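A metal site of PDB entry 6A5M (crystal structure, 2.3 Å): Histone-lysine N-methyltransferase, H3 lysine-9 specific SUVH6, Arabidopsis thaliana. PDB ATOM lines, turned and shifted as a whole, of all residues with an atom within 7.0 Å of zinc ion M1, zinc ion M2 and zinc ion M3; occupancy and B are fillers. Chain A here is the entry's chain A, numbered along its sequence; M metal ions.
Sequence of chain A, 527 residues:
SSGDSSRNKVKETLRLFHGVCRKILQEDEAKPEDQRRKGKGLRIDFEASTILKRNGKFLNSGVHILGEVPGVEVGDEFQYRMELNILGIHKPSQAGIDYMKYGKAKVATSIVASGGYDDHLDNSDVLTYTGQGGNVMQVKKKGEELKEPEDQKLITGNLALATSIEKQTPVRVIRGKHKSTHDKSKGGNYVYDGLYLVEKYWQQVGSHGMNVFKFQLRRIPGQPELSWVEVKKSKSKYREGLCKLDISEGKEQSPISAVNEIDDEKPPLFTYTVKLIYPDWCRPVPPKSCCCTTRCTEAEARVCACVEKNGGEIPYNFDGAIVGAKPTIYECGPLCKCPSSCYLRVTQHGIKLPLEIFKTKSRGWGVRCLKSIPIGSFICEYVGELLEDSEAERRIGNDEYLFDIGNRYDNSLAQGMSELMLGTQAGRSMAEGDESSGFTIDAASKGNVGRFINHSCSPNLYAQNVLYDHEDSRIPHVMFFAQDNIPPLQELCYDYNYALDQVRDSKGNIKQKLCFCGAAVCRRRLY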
ATOM      1  N   LYS A 288       1.048  13.009 -14.788  1.00  0.00           N
ATOM      2  CA  LYS A 288      -0.190  12.470 -15.329  1.00  0.00           C
ATOM      3  C   LYS A 288      -0.131  12.527 -16.837  1.00  0.00           C
ATOM      4  O   LYS A 288       0.215  13.546 -17.420  1.00  0.00           O
ATOM      5  CB  LYS A 288      -1.420  13.240 -14.798  1.00  0.00           C
ATOM      6  CG  LYS A 288      -1.371  13.607 -13.285  1.00  0.00           C
ATOM      7  CD  LYS A 288      -0.742  12.561 -12.348  1.00  0.00           C
ATOM      8  CE  LYS A 288      -1.188  11.123 -12.606  1.00  0.00           C
ATOM      9  NZ  LYS A 288      -0.157  10.174 -12.110  1.00  0.00           N
ATOM     10  N   SER A 289      -0.403  11.347 -17.400  1.00  0.00           N
ATOM     11  CA  SER A 289      -0.091  10.954 -18.752  1.00  0.00           C
ATOM     12  C   SER A 289      -1.174  11.283 -19.758  1.00  0.00           C
ATOM     13  O   SER A 289      -2.105  12.050 -19.481  1.00  0.00           O
ATOM     14  CB  SER A 289       0.221   9.456 -18.815  1.00  0.00           C
ATOM     15  OG  SER A 289      -0.952   8.690 -18.995  1.00  0.00           O
ATOM     16  N   CYS A 290      -1.058  10.671 -20.927  1.00  0.00           N
ATOM     17  CA  CYS A 290      -1.859  11.035 -22.079  1.00  0.00           C
ATOM     18  C   CYS A 290      -2.563   9.854 -22.714  1.00  0.00           C
ATOM     19  O   CYS A 290      -2.085   8.722 -22.655  1.00  0.00           O
ATOM     20  CB  CYS A 290      -0.977  11.723 -23.102  1.00  0.00           C
ATOM     21  SG  CYS A 290      -1.907  12.722 -24.265  1.00  0.00           S
ATOM     22  N   CYS A 291      -3.703  10.128 -23.336  1.00  0.00           N
ATOM     23  CA  CYS A 291      -4.491   9.087 -23.987  1.00  0.00           C
ATOM     24  C   CYS A 291      -4.775   9.491 -25.429  1.00  0.00           C
ATOM     25  O   CYS A 291      -5.900   9.844 -25.788  1.00  0.00           O
ATOM     26  CB  CYS A 291      -5.796   8.861 -23.235  1.00  0.00           C
ATOM     27  SG  CYS A 291      -5.692   7.626 -21.912  1.00  0.00           S
ATOM     28  N   CYS A 292      -3.739   9.425 -26.254  1.00  0.00           N
ATOM     29  CA  CYS A 292      -3.820   9.729 -27.676  1.00  0.00           C
ATOM     30  C   CYS A 292      -2.802   8.828 -28.359  1.00  0.00           C
ATOM     31  O   CYS A 292      -1.649   8.777 -27.966  1.00  0.00           O
ATOM     32  CB  CYS A 292      -3.520  11.213 -27.943  1.00  0.00           C
ATOM     33  SG  CYS A 292      -4.392  12.419 -26.882  1.00  0.00           S
ATOM     34  N   THR A 293      -3.248   8.092 -29.375  1.00  0.00           N
ATOM     35  CA  THR A 293      -2.362   7.146 -30.045  1.00  0.00           C
ATOM     36  C   THR A 293      -1.556   7.809 -31.152  1.00  0.00           C
ATOM     37  O   THR A 293      -0.660   7.208 -31.732  1.00  0.00           O
ATOM     38  CB  THR A 293      -3.123   5.965 -30.622  1.00  0.00           C
ATOM     39  OG1 THR A 293      -2.195   4.977 -31.087  1.00  0.00           O
ATOM     40  CG2 THR A 293      -4.006   6.420 -31.777  1.00  0.00           C
ATOM     41  N   THR A 294      -1.903   9.057 -31.460  1.00  0.00           N
ATOM     42  CA  THR A 294      -1.172   9.796 -32.461  1.00  0.00           C
ATOM     43  C   THR A 294      -0.860  11.203 -31.976  1.00  0.00           C
ATOM     44  O   THR A 294      -1.133  11.530 -30.821  1.00  0.00           O
ATOM     45  CB  THR A 294      -1.945   9.880 -33.761  1.00  0.00           C
ATOM     46  OG1 THR A 294      -1.132  10.535 -34.735  1.00  0.00           O
ATOM     47  CG2 THR A 294      -3.237  10.673 -33.553  1.00  0.00           C
ATOM     48  N   ARG A 295      -0.305  12.037 -32.853  1.00  0.00           N
ATOM     49  CA  ARG A 295       0.045  13.411 -32.480  1.00  0.00           C
ATOM     50  C   ARG A 295      -1.113  14.140 -31.819  1.00  0.00           C
ATOM     51  O   ARG A 295      -2.222  14.164 -32.348  1.00  0.00           O
ATOM     52  CB  ARG A 295       0.511  14.228 -33.695  1.00  0.00           C
ATOM     53  CG  ARG A 295       1.568  13.579 -34.564  1.00  0.00           C
ATOM     54  CD  ARG A 295       1.984  14.546 -35.649  1.00  0.00           C
ATOM     55  NE  ARG A 295       3.125  14.069 -36.420  1.00  0.00           N
ATOM     56  CZ  ARG A 295       3.860  14.827 -37.228  1.00  0.00           C
ATOM     57  NH1 ARG A 295       4.867  14.305 -37.894  1.00  0.00           N
ATOM     58  NH2 ARG A 295       3.574  16.115 -37.364  1.00  0.00           N
ATOM     59  N   CYS A 296      -0.846  14.730 -30.661  1.00  0.00           N
ATOM     60  CA  CYS A 296      -1.871  15.480 -29.940  1.00  0.00           C
ATOM     61  C   CYS A 296      -2.161  16.790 -30.625  1.00  0.00           C
ATOM     62  O   CYS A 296      -1.251  17.516 -31.030  1.00  0.00           O
ATOM     63  CB  CYS A 296      -1.464  15.748 -28.504  1.00  0.00           C
ATOM     64  SG  CYS A 296      -1.252  14.256 -27.581  1.00  0.00           S
ATOM     65  N   THR A 297      -3.453  17.041 -30.769  1.00  0.00           N
ATOM     66  CA  THR A 297      -3.980  18.246 -31.331  1.00  0.00           C
ATOM     67  C   THR A 297      -5.359  18.562 -30.756  1.00  0.00           C
ATOM     68  O   THR A 297      -6.063  17.673 -30.348  1.00  0.00           O
ATOM     69  CB  THR A 297      -4.013  18.152 -32.853  1.00  0.00           C
ATOM     70  OG1 THR A 297      -4.938  19.097 -33.383  1.00  0.00           O
ATOM     71  CG2 THR A 297      -4.442  16.810 -33.299  1.00  0.00           C
ATOM     72  N   VAL A 303     -10.544  13.540 -25.501  1.00  0.00           N
ATOM     73  CA  VAL A 303      -9.796  14.331 -24.532  1.00  0.00           C
ATOM     74  C   VAL A 303      -8.291  14.089 -24.555  1.00  0.00           C
ATOM     75  O   VAL A 303      -7.849  12.968 -24.495  1.00  0.00           O
ATOM     76  CB  VAL A 303     -10.319  14.066 -23.103  1.00  0.00           C
ATOM     77  CG1 VAL A 303      -9.461  14.760 -22.044  1.00  0.00           C
ATOM     78  CG2 VAL A 303     -11.744  14.536 -22.972  1.00  0.00           C
ATOM     79  N   CYS A 304      -7.520  15.162 -24.574  1.00  0.00           N
ATOM     80  CA  CYS A 304      -6.095  15.069 -24.299  1.00  0.00           C
ATOM     81  C   CYS A 304      -5.775  15.879 -23.040  1.00  0.00           C
ATOM     82  O   CYS A 304      -5.904  17.103 -23.031  1.00  0.00           O
ATOM     83  CB  CYS A 304      -5.253  15.585 -25.477  1.00  0.00           C
ATOM     84  SG  CYS A 304      -3.474  15.629 -25.125  1.00  0.00           S
ATOM     85  N   ALA A 305      -5.382  15.175 -21.979  1.00  0.00           N
ATOM     86  CA  ALA A 305      -5.089  15.796 -20.685  1.00  0.00           C
ATOM     87  C   ALA A 305      -3.991  16.843 -20.792  1.00  0.00           C
ATOM     88  O   ALA A 305      -4.017  17.871 -20.117  1.00  0.00           O
ATOM     89  CB  ALA A 305      -4.679  14.737 -19.686  1.00  0.00           C
ATOM     90  N   CYS A 306      -3.016  16.580 -21.654  1.00  0.00           N
ATOM     91  CA  CYS A 306      -1.882  17.476 -21.781  1.00  0.00           C
ATOM     92  C   CYS A 306      -2.286  18.794 -22.437  1.00  0.00           C
ATOM     93  O   CYS A 306      -1.729  19.841 -22.117  1.00  0.00           O
ATOM     94  CB  CYS A 306      -0.759  16.767 -22.545  1.00  0.00           C
ATOM     95  SG  CYS A 306      -0.234  15.246 -21.676  1.00  0.00           S
ATOM     96  N   VAL A 307      -3.283  18.770 -23.318  1.00  0.00           N
ATOM     97  CA  VAL A 307      -3.839  20.006 -23.872  1.00  0.00           C
ATOM     98  C   VAL A 307      -4.587  20.819 -22.807  1.00  0.00           C
ATOM     99  O   VAL A 307      -4.568  22.059 -22.837  1.00  0.00           O
ATOM    100  CB  VAL A 307      -4.793  19.717 -25.056  1.00  0.00           C
ATOM    101  CG1 VAL A 307      -5.480  20.989 -25.537  1.00  0.00           C
ATOM    102  CG2 VAL A 307      -4.037  19.042 -26.189  1.00  0.00           C
ATOM    103  N   LYS A 309      -3.794  20.730 -19.624  1.00  0.00           N
ATOM    104  CA  LYS A 309      -2.722  21.270 -18.787  1.00  0.00           C
ATOM    105  C   LYS A 309      -2.273  22.637 -19.307  1.00  0.00           C
ATOM    106  O   LYS A 309      -1.931  23.521 -18.534  1.00  0.00           O
ATOM    107  CB  LYS A 309      -1.524  20.326 -18.748  1.00  0.00           C
ATOM    108  CG  LYS A 309      -1.647  19.171 -17.778  1.00  0.00           C
ATOM    109  CD  LYS A 309      -0.421  18.260 -17.899  1.00  0.00           C
ATOM    110  CE  LYS A 309      -0.707  16.875 -17.316  1.00  0.00           C
ATOM    111  NZ  LYS A 309       0.415  15.935 -17.579  1.00  0.00           N
ATOM    112  N   GLU A 331       4.619  19.679 -21.866  1.00  0.00           N
ATOM    113  CA  GLU A 331       4.805  18.788 -22.998  1.00  0.00           C
ATOM    114  C   GLU A 331       4.352  17.372 -22.621  1.00  0.00           C
ATOM    115  O   GLU A 331       4.230  17.059 -21.433  1.00  0.00           O
ATOM    116  CB  GLU A 331       6.275  18.773 -23.457  1.00  0.00           C
ATOM    117  CG  GLU A 331       6.677  19.990 -24.328  1.00  0.00           C
ATOM    118  CD  GLU A 331       8.116  19.902 -24.842  1.00  0.00           C
ATOM    119  OE1 GLU A 331       8.658  18.781 -24.915  1.00  0.00           O
ATOM    120  OE2 GLU A 331       8.713  20.942 -25.172  1.00  0.00           O
ATOM    121  N   CYS A 332       4.102  16.533 -23.610  1.00  0.00           N
ATOM    122  CA  CYS A 332       3.762  15.149 -23.340  1.00  0.00           C
ATOM    123  C   CYS A 332       4.980  14.448 -22.769  1.00  0.00           C
ATOM    124  O   CYS A 332       6.114  14.774 -23.123  1.00  0.00           O
ATOM    125  CB  CYS A 332       3.268  14.431 -24.609  1.00  0.00           C
ATOM    126  SG  CYS A 332       1.605  14.953 -25.077  1.00  0.00           S
ATOM    127  N   GLY A 333       4.734  13.498 -21.861  1.00  0.00           N
ATOM    128  CA  GLY A 333       5.796  12.905 -21.072  1.00  0.00           C
ATOM    129  C   GLY A 333       6.101  11.476 -21.476  1.00  0.00           C
ATOM    130  O   GLY A 333       5.719  11.041 -22.562  1.00  0.00           O
ATOM    131  N   LEU A 335       5.081   8.591 -20.374  1.00  0.00           N
ATOM    132  CA  LEU A 335       4.008   7.619 -20.370  1.00  0.00           C
ATOM    133  C   LEU A 335       2.804   8.090 -21.195  1.00  0.00           C
ATOM    134  O   LEU A 335       1.750   7.463 -21.129  1.00  0.00           O
ATOM    135  CB  LEU A 335       3.574   7.293 -18.941  1.00  0.00           C
ATOM    136  CG  LEU A 335       4.638   6.634 -18.059  1.00  0.00           C
ATOM    137  CD1 LEU A 335       4.022   6.120 -16.775  1.00  0.00           C
ATOM    138  CD2 LEU A 335       5.341   5.526 -18.798  1.00  0.00           C
ATOM    139  N   CYS A 336       2.942   9.176 -21.945  1.00  0.00           N
ATOM    140  CA  CYS A 336       1.944   9.503 -22.974  1.00  0.00           C
ATOM    141  C   CYS A 336       2.098   8.537 -24.159  1.00  0.00           C
ATOM    142  O   CYS A 336       3.226   8.274 -24.597  1.00  0.00           O
ATOM    143  CB  CYS A 336       2.070  10.960 -23.435  1.00  0.00           C
ATOM    144  SG  CYS A 336       1.746  12.206 -22.172  1.00  0.00           S
ATOM    145  N   LYS A 337       1.002   8.011 -24.676  1.00  0.00           N
ATOM    146  CA  LYS A 337       1.064   7.019 -25.760  1.00  0.00           C
ATOM    147  C   LYS A 337       1.321   7.655 -27.132  1.00  0.00           C
ATOM    148  O   LYS A 337       1.340   6.984 -28.162  1.00  0.00           O
ATOM    149  CB  LYS A 337      -0.214   6.195 -25.771  1.00  0.00           C
ATOM    150  CG  LYS A 337      -0.604   5.674 -24.389  1.00  0.00           C
ATOM    151  CD  LYS A 337      -1.967   5.015 -24.397  1.00  0.00           C
ATOM    152  CE  LYS A 337      -2.296   4.402 -23.058  1.00  0.00           C
ATOM    153  NZ  LYS A 337      -3.747   4.080 -22.943  1.00  0.00           N
ATOM    154  N   CYS A 338       1.578   8.957 -27.096  1.00  0.00           N
ATOM    155  CA  CYS A 338       1.913   9.705 -28.301  1.00  0.00           C
ATOM    156  C   CYS A 338       3.213   9.265 -28.906  1.00  0.00           C
ATOM    157  O   CYS A 338       4.140   8.856 -28.216  1.00  0.00           O
ATOM    158  CB  CYS A 338       2.039  11.192 -27.983  1.00  0.00           C
ATOM    159  SG  CYS A 338       0.593  11.839 -27.168  1.00  0.00           S
ATOM    160  N   PRO A 339       3.275   9.383 -30.223  1.00  0.00           N
ATOM    161  CA  PRO A 339       4.524   9.149 -30.947  1.00  0.00           C
ATOM    162  C   PRO A 339       5.501  10.287 -30.675  1.00  0.00           C
ATOM    163  O   PRO A 339       5.094  11.329 -30.180  1.00  0.00           O
ATOM    164  CB  PRO A 339       4.083   9.124 -32.407  1.00  0.00           C
ATOM    165  CG  PRO A 339       2.908  10.030 -32.431  1.00  0.00           C
ATOM    166  CD  PRO A 339       2.194   9.797 -31.127  1.00  0.00           C
ATOM    167  N   CYS A 342       4.631  13.924 -31.836  1.00  0.00           N
ATOM    168  CA  CYS A 342       3.528  14.688 -31.258  1.00  0.00           C
ATOM    169  C   CYS A 342       3.868  16.184 -31.199  1.00  0.00           C
ATOM    170  O   CYS A 342       5.023  16.563 -30.968  1.00  0.00           O
ATOM    171  CB  CYS A 342       3.187  14.180 -29.857  1.00  0.00           C
ATOM    172  SG  CYS A 342       1.985  15.206 -28.977  1.00  0.00           S
ATOM    173  N   TYR A 343       2.853  17.026 -31.414  1.00  0.00           N
ATOM    174  CA  TYR A 343       3.068  18.479 -31.481  1.00  0.00           C
ATOM    175  C   TYR A 343       3.419  19.062 -30.109  1.00  0.00           C
ATOM    176  O   TYR A 343       3.924  20.189 -30.008  1.00  0.00           O
ATOM    177  CB  TYR A 343       1.829  19.182 -32.040  1.00  0.00           C
ATOM    178  CG  TYR A 343       1.483  18.802 -33.480  1.00  0.00           C
ATOM    179  CD1 TYR A 343       2.402  19.008 -34.507  1.00  0.00           C
ATOM    180  CD2 TYR A 343       0.244  18.267 -33.795  1.00  0.00           C
ATOM    181  CE1 TYR A 343       2.096  18.668 -35.822  1.00  0.00           C
ATOM    182  CE2 TYR A 343      -0.077  17.927 -35.110  1.00  0.00           C
ATOM    183  CZ  TYR A 343       0.856  18.131 -36.120  1.00  0.00           C
ATOM    184  OH  TYR A 343       0.549  17.806 -37.421  1.00  0.00           O
ATOM    185  N   LEU A 344       3.122  18.286 -29.069  1.00  0.00           N
ATOM    186  CA  LEU A 344       3.441  18.646 -27.701  1.00  0.00           C
ATOM    187  C   LEU A 344       4.762  18.026 -27.278  1.00  0.00           C
ATOM    188  O   LEU A 344       5.033  17.925 -26.098  1.00  0.00           O
ATOM    189  CB  LEU A 344       2.337  18.176 -26.745  1.00  0.00           C
ATOM    190  CG  LEU A 344       1.084  19.048 -26.657  1.00  0.00           C
ATOM    191  CD1 LEU A 344       0.377  18.818 -25.342  1.00  0.00           C
ATOM    192  CD2 LEU A 344       1.484  20.499 -26.787  1.00  0.00           C
ATOM    193  N   ARG A 345       5.555  17.587 -28.238  1.00  0.00           N
ATOM    194  CA  ARG A 345       6.886  17.076 -27.927  1.00  0.00           C
ATOM    195  C   ARG A 345       7.916  17.879 -28.707  1.00  0.00           C
ATOM    196  O   ARG A 345       8.115  17.634 -29.901  1.00  0.00           O
ATOM    197  CB  ARG A 345       7.016  15.585 -28.257  1.00  0.00           C
ATOM    198  CG  ARG A 345       6.161  14.645 -27.414  1.00  0.00           C
ATOM    199  CD  ARG A 345       6.487  13.218 -27.789  1.00  0.00           C
ATOM    200  NE  ARG A 345       5.596  12.204 -27.232  1.00  0.00           N
ATOM    201  CZ  ARG A 345       5.769  11.618 -26.045  1.00  0.00           C
ATOM    202  NH1 ARG A 345       6.788  11.958 -25.256  1.00  0.00           N
ATOM    203  NH2 ARG A 345       4.897  10.689 -25.648  1.00  0.00           N
HETATM  204 ZN    ZN M   1      -2.595  13.786 -25.995  1.00  0.00          ZN
HETATM  205 ZN    ZN M   2       0.353  13.735 -23.351  1.00  0.00          ZN
HETATM  206 ZN    ZN M   3       1.192  13.988 -27.145  1.00  0.00          ZN
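Zinc ion M1 is bound by the side-chain sulfur of Cys 296, the side-chain sulfur of Cys 290, the side-chain sulfur of Cys 304 and the side-chain sulfur of Cys 292.
Zinc ion M2 is bound by the side-chain sulfur (SG) of Cys 306, the side-chain sulfur (SG) of Cys 336, the side-chain sulfur (SG) of Cys 332 and the side-chain sulfur (SG) of Cys 290.
SG of Cys 304 sits close to N of Cys 306 (3.6 Å). The side-chain sulfur (SG) of Cys 304 lies close to the backbone NH (N) of Val 307 (3.6 Å). O of Cys 292 sits at hydrogen-bond distance from N of Cys 338. The backbone carbonyl oxygen (O) of Cys 338 lies within hydrogen-bond range of the guanidinium group (NH2) of Arg 345 (3.2 Å). The backbone NH of Cys 332 lies within hydrogen-bond range of the backbone carbonyl oxygen of Leu 344, 3.0 Å away. SG of Cys 342 sits close to N of Leu 344 (3.3 Å). The side-chain sulfur of Cys 336 sits close to the backbone NH of Gly 333, at 3.3 Å. O of Cys 336 lies within hydrogen-bond range of NH2 of Arg 345, at 3.1 Å.
Five residues have an atom within 4 Å of zinc ion M1: Cys 290, Cys 292, Cys 296, Cys 304 and Cys 338. The nearest printed residue that does not touch zinc ion M1 is Cys 332 (4.5 Å).
Zinc ion M3 is bound by SG of Cys 338, SG of Cys 332, SG of Cys 342 and SG of Cys 296. Zinc ion M3 has four donor atoms within binding distance.
Of the 28 residues printed, 4 come within 4 Å of zinc ion M2.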
